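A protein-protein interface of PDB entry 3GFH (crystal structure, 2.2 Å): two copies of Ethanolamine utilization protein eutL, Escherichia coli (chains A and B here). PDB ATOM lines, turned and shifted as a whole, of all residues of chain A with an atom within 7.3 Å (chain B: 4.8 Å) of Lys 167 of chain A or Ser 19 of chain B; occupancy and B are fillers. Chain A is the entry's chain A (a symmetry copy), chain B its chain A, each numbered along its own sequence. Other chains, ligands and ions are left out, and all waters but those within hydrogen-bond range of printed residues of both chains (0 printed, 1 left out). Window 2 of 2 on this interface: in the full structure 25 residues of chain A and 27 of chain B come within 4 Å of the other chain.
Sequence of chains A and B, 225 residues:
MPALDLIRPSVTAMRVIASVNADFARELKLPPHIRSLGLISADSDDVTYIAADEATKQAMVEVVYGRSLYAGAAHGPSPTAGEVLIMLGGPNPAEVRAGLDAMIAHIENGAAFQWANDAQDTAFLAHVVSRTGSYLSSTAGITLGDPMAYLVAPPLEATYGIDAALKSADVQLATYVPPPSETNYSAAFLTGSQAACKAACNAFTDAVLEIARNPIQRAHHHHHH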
ATOM      1  N   TYR A 160     -33.477  15.100  10.021  1.00  0.00           N
ATOM      2  CA  TYR A 160     -33.186  13.888  10.744  1.00  0.00           C
ATOM      3  C   TYR A 160     -32.838  12.815   9.756  1.00  0.00           C
ATOM      4  O   TYR A 160     -31.695  12.356   9.668  1.00  0.00           O
ATOM      5  CB  TYR A 160     -34.467  13.482  11.494  1.00  0.00           C
ATOM      6  CG  TYR A 160     -34.299  12.551  12.695  1.00  0.00           C
ATOM      7  CD1 TYR A 160     -33.603  12.959  13.819  1.00  0.00           C
ATOM      8  CD2 TYR A 160     -34.882  11.266  12.714  1.00  0.00           C
ATOM      9  CE1 TYR A 160     -33.470  12.122  14.913  1.00  0.00           C
ATOM     10  CE2 TYR A 160     -34.722  10.405  13.828  1.00  0.00           C
ATOM     11  CZ  TYR A 160     -34.033  10.865  14.912  1.00  0.00           C
ATOM     12  OH  TYR A 160     -33.868  10.120  16.038  1.00  0.00           O
ATOM     13  N   GLY A 161     -33.847  12.445   8.966  1.00  0.00           N
ATOM     14  CA  GLY A 161     -33.639  11.547   7.863  1.00  0.00           C
ATOM     15  C   GLY A 161     -32.366  11.852   7.091  1.00  0.00           C
ATOM     16  O   GLY A 161     -31.745  10.944   6.649  1.00  0.00           O
ATOM     17  N   ILE A 162     -31.972  13.103   6.908  1.00  0.00           N
ATOM     18  CA  ILE A 162     -30.725  13.373   6.131  1.00  0.00           C
ATOM     19  C   ILE A 162     -29.555  12.852   6.905  1.00  0.00           C
ATOM     20  O   ILE A 162     -28.820  11.972   6.441  1.00  0.00           O
ATOM     21  CB  ILE A 162     -30.477  14.859   5.882  1.00  0.00           C
ATOM     22  CG1 ILE A 162     -31.476  15.413   4.895  1.00  0.00           C
ATOM     23  CG2 ILE A 162     -29.086  15.103   5.267  1.00  0.00           C
ATOM     24  CD1 ILE A 162     -31.223  16.895   4.623  1.00  0.00           C
ATOM     25  N   ASP A 163     -29.417  13.350   8.127  1.00  0.00           N
ATOM     26  CA  ASP A 163     -28.368  12.878   9.012  1.00  0.00           C
ATOM     27  C   ASP A 163     -28.331  11.354   8.961  1.00  0.00           C
ATOM     28  O   ASP A 163     -27.300  10.755   8.724  1.00  0.00           O
ATOM     29  CB  ASP A 163     -28.647  13.377  10.451  1.00  0.00           C
ATOM     30  CG  ASP A 163     -27.529  13.043  11.428  1.00  0.00           C
ATOM     31  OD1 ASP A 163     -26.344  13.425  11.199  1.00  0.00           O
ATOM     32  OD2 ASP A 163     -27.849  12.391  12.442  1.00  0.00           O
ATOM     33  N   ALA A 164     -29.482  10.727   9.175  1.00  0.00           N
ATOM     34  CA  ALA A 164     -29.574   9.277   9.169  1.00  0.00           C
ATOM     35  C   ALA A 164     -28.920   8.689   7.933  1.00  0.00           C
ATOM     36  O   ALA A 164     -28.225   7.694   8.015  1.00  0.00           O
ATOM     37  CB  ALA A 164     -31.060   8.839   9.243  1.00  0.00           C
ATOM     38  N   ALA A 165     -29.195   9.287   6.775  1.00  0.00           N
ATOM     39  CA  ALA A 165     -28.720   8.756   5.489  1.00  0.00           C
ATOM     40  C   ALA A 165     -27.180   8.807   5.338  1.00  0.00           C
ATOM     41  O   ALA A 165     -26.522   7.781   5.043  1.00  0.00           O
ATOM     42  CB  ALA A 165     -29.411   9.515   4.340  1.00  0.00           C
ATOM     43  N   LEU A 166     -26.595   9.978   5.586  1.00  0.00           N
ATOM     44  CA  LEU A 166     -25.123  10.086   5.602  1.00  0.00           C
ATOM     45  C   LEU A 166     -24.519   9.011   6.513  1.00  0.00           C
ATOM     46  O   LEU A 166     -23.491   8.420   6.201  1.00  0.00           O
ATOM     47  CB  LEU A 166     -24.726  11.470   6.052  1.00  0.00           C
ATOM     48  CG  LEU A 166     -25.467  12.433   5.151  1.00  0.00           C
ATOM     49  CD1 LEU A 166     -25.322  13.828   5.615  1.00  0.00           C
ATOM     50  CD2 LEU A 166     -24.934  12.243   3.756  1.00  0.00           C
ATOM     51  N   LYS A 167     -25.201   8.712   7.612  1.00  0.00           N
ATOM     52  CA  LYS A 167     -24.689   7.733   8.569  1.00  0.00           C
ATOM     53  C   LYS A 167     -24.828   6.266   8.104  1.00  0.00           C
ATOM     54  O   LYS A 167     -24.186   5.366   8.669  1.00  0.00           O
ATOM     55  CB  LYS A 167     -25.369   7.929   9.911  1.00  0.00           C
ATOM     56  CG  LYS A 167     -24.963   9.238  10.598  1.00  0.00           C
ATOM     57  CD  LYS A 167     -25.872   9.545  11.800  1.00  0.00           C
ATOM     58  CE  LYS A 167     -25.234  10.572  12.753  1.00  0.00           C
ATOM     59  NZ  LYS A 167     -25.957  10.659  14.085  1.00  0.00           N
ATOM     60  N   SER A 168     -25.646   6.050   7.072  1.00  0.00           N
ATOM     61  CA  SER A 168     -26.004   4.711   6.608  1.00  0.00           C
ATOM     62  C   SER A 168     -25.262   4.317   5.328  1.00  0.00           C
ATOM     63  O   SER A 168     -25.162   3.134   4.956  1.00  0.00           O
ATOM     64  CB  SER A 168     -27.527   4.643   6.356  1.00  0.00           C
ATOM     65  OG  SER A 168     -27.998   5.598   5.373  1.00  0.00           O
ATOM     66  N   ALA A 169     -24.729   5.294   4.627  1.00  0.00           N
ATOM     67  CA  ALA A 169     -24.086   4.943   3.395  1.00  0.00           C
ATOM     68  C   ALA A 169     -23.129   6.035   3.048  1.00  0.00           C
ATOM     69  O   ALA A 169     -23.396   7.202   3.367  1.00  0.00           O
ATOM     70  CB  ALA A 169     -25.118   4.796   2.334  1.00  0.00           C
ATOM     71  N   ASP A 170     -22.003   5.681   2.432  1.00  0.00           N
ATOM     72  CA  ASP A 170     -21.070   6.719   2.060  1.00  0.00           C
ATOM     73  C   ASP A 170     -21.719   7.332   0.851  1.00  0.00           C
ATOM     74  O   ASP A 170     -21.867   6.697  -0.215  1.00  0.00           O
ATOM     75  CB  ASP A 170     -19.635   6.241   1.759  1.00  0.00           C
ATOM     76  CG  ASP A 170     -19.598   5.209   0.714  1.00  0.00           C
ATOM     77  OD1 ASP A 170     -18.530   4.987   0.083  1.00  0.00           O
ATOM     78  OD2 ASP A 170     -20.674   4.634   0.514  1.00  0.00           O
ATOM     79  N   VAL A 171     -22.141   8.569   1.087  1.00  0.00           N
ATOM     80  CA  VAL A 171     -22.685   9.423   0.083  1.00  0.00           C
ATOM     81  C   VAL A 171     -22.140  10.793   0.375  1.00  0.00           C
ATOM     82  O   VAL A 171     -21.443  11.020   1.382  1.00  0.00           O
ATOM     83  CB  VAL A 171     -24.205   9.408   0.089  1.00  0.00           C
ATOM     84  CG1 VAL A 171     -24.683   8.283  -0.728  1.00  0.00           C
ATOM     85  CG2 VAL A 171     -24.750   9.250   1.501  1.00  0.00           C
ATOM     86  N   ALA A 203     -32.598   4.553   4.697  1.00  0.00           N
ATOM     87  CA  ALA A 203     -32.584   5.021   6.090  1.00  0.00           C
ATOM     88  C   ALA A 203     -33.416   6.288   6.170  1.00  0.00           C
ATOM     89  O   ALA A 203     -34.098   6.531   7.142  1.00  0.00           O
ATOM     90  CB  ALA A 203     -31.153   5.281   6.577  1.00  0.00           C
ATOM     91  N   ILE B  17     -30.584  14.597  17.713  1.00  0.00           N
ATOM     92  CA  ILE B  17     -29.542  13.834  17.083  1.00  0.00           C
ATOM     93  C   ILE B  17     -28.459  13.924  18.119  1.00  0.00           C
ATOM     94  O   ILE B  17     -27.920  14.995  18.321  1.00  0.00           O
ATOM     95  CB  ILE B  17     -29.099  14.509  15.771  1.00  0.00           C
ATOM     96  CG1 ILE B  17     -30.333  14.711  14.880  1.00  0.00           C
ATOM     97  CG2 ILE B  17     -27.979  13.730  15.088  1.00  0.00           C
ATOM     98  CD1 ILE B  17     -30.068  15.342  13.524  1.00  0.00           C
ATOM     99  N   ALA B  18     -28.149  12.815  18.799  1.00  0.00           N
ATOM    100  CA  ALA B  18     -27.116  12.852  19.838  1.00  0.00           C
ATOM    101  C   ALA B  18     -25.798  13.346  19.237  1.00  0.00           C
ATOM    102  O   ALA B  18     -25.106  14.186  19.866  1.00  0.00           O
ATOM    103  CB  ALA B  18     -26.948  11.498  20.502  1.00  0.00           C
ATOM    104  N   SER B  19     -25.511  12.897  17.997  1.00  0.00           N
ATOM    105  CA  SER B  19     -24.215  13.125  17.371  1.00  0.00           C
ATOM    106  C   SER B  19     -24.239  13.337  15.846  1.00  0.00           C
ATOM    107  O   SER B  19     -24.060  12.386  15.078  1.00  0.00           O
ATOM    108  CB  SER B  19     -23.287  11.931  17.682  1.00  0.00           C
ATOM    109  OG  SER B  19     -22.011  12.097  17.040  1.00  0.00           O
ATOM    110  N   VAL B  20     -24.366  14.587  15.408  1.00  0.00           N
ATOM    111  CA  VAL B  20     -24.499  14.887  13.989  1.00  0.00           C
ATOM    112  C   VAL B  20     -23.423  14.192  13.127  1.00  0.00           C
ATOM    113  O   VAL B  20     -22.268  14.098  13.506  1.00  0.00           O
ATOM    114  CB  VAL B  20     -24.436  16.391  13.733  1.00  0.00           C
ATOM    115  CG1 VAL B  20     -25.671  17.115  14.322  1.00  0.00           C
ATOM    116  CG2 VAL B  20     -23.175  16.992  14.365  1.00  0.00           C
ATOM    117  N   ASN B  21     -23.806  13.678  11.968  1.00  0.00           N
ATOM    118  CA  ASN B  21     -22.802  13.240  11.012  1.00  0.00           C
ATOM    119  C   ASN B  21     -21.869  14.411  10.714  1.00  0.00           C
ATOM    120  O   ASN B  21     -22.301  15.548  10.604  1.00  0.00           O
ATOM    121  CB  ASN B  21     -23.467  12.792   9.713  1.00  0.00           C
ATOM    122  CG  ASN B  21     -22.473  12.583   8.610  1.00  0.00           C
ATOM    123  OD1 ASN B  21     -21.819  11.556   8.561  1.00  0.00           O
ATOM    124  ND2 ASN B  21     -22.329  13.580   7.721  1.00  0.00           N
ATOM    125  N   ARG B  35     -21.880  19.476  19.094  1.00  0.00           N
ATOM    126  CA  ARG B  35     -21.992  18.215  18.370  1.00  0.00           C
ATOM    127  C   ARG B  35     -23.348  17.514  18.556  1.00  0.00           C
ATOM    128  O   ARG B  35     -23.576  16.465  17.987  1.00  0.00           O
ATOM    129  CB  ARG B  35     -20.844  17.270  18.704  1.00  0.00           C
ATOM    130  CG  ARG B  35     -19.725  17.362  17.674  1.00  0.00           C
ATOM    131  CD  ARG B  35     -19.258  18.804  17.556  1.00  0.00           C
ATOM    132  NE  ARG B  35     -18.506  19.070  16.335  1.00  0.00           N
ATOM    133  CZ  ARG B  35     -18.963  18.814  15.118  1.00  0.00           C
ATOM    134  NH1 ARG B  35     -20.156  18.250  14.969  1.00  0.00           N
ATOM    135  NH2 ARG B  35     -18.227  19.107  14.055  1.00  0.00           N
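The side-chain amino group of Lys 167 of chain A lies within salt-bridge range of the side-chain carboxylate of Asp 163 of chain A (3.0 Å).
The backbone NH (N) of Val 20 of chain B is in hydrogen-bond range of the backbone carbonyl oxygen (O) of Arg 35 of chain B (3.3 Å).
Of the 6 printed residues of chain B, 4 touch a printed residue of chain A.
Hydrophobic or aromatic side chains of chain B that line the printed part of chain A: Ile 17.
Of the 13 printed residues of chain A, 4 touch a printed residue of chain B.
Printed residues of chain A that touch a printed residue of chain B: Tyr 160, Asp 163, Leu 166 and Lys 167.
Hydrophobic or aromatic side chains of chain A within 4 Å of the printed part of chain B: Tyr 160 and Leu 166.
No position is printed for both chains.
Of the 8 pairs that touch across the chains among the printed residues, none has its exchanged pair printed and touching as well.
Of the printed residues of chain B, Tyr 160 of chain A touches Ile 17 (3.9 Å).
Printed residues of chain B within 4 Å of Leu 166 of chain A: Asn 21.
Of chain B, only Ile 17 (3.8 Å), Ser 19 (2.8 Å) and Asn 21 (3.5 Å) come within 4 Å of Lys 167 of chain A.
Ala 169 of chain A touches none of the printed residues of chain B.
Val 171 of chain A touches none of the printed residues of chain B.
Printed residues of chain A within 4 Å of Ile 17 of chain B: Tyr 160, Asp 163 and Lys 167.
No residue of chain A comes within 4 Å of Ala 18 of chain B.
Ser 19 of chain B touches just one residue of chain A: Lys 167 (2.8 Å).
Printed residues of chain A within 4 Å of Val 20 of chain B: Asp 163 (3.6 Å).
The nearest residue of chain A that does not touch Ser 19 of chain B is Asp 163 of chain A (4.6 Å).
The nearest printed residue of chain A that does not touch Ile 17 of chain B is Ala 164 of chain A (6.4 Å).
O of Ser 19 of chain B lies within hydrogen-bond range of NZ of Lys 167 of chain A (2.8 Å).
The backbone NH (N) of Asn 21 of chain B is in hydrogen-bond range of the side-chain carboxylate (OD1) of Asp 163 of chain A, at 2.7 Å.
Among the printed residues, merely in contact across the chains: Asp 163 of chain A with Ile 17 of chain B (3.0 Å), Lys 167 of chain A with Asn 21 of chain B (3.5 Å), Asp 163 of chain A with Val 20 of chain B (3.6 Å), Leu 166 of chain A with Asn 21 of chain B (3.6 Å), Lys 167 of chain A with Ile 17 of chain B (3.8 Å) and Tyr 160 of chain A with Ile 17 of chain B (3.9 Å).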
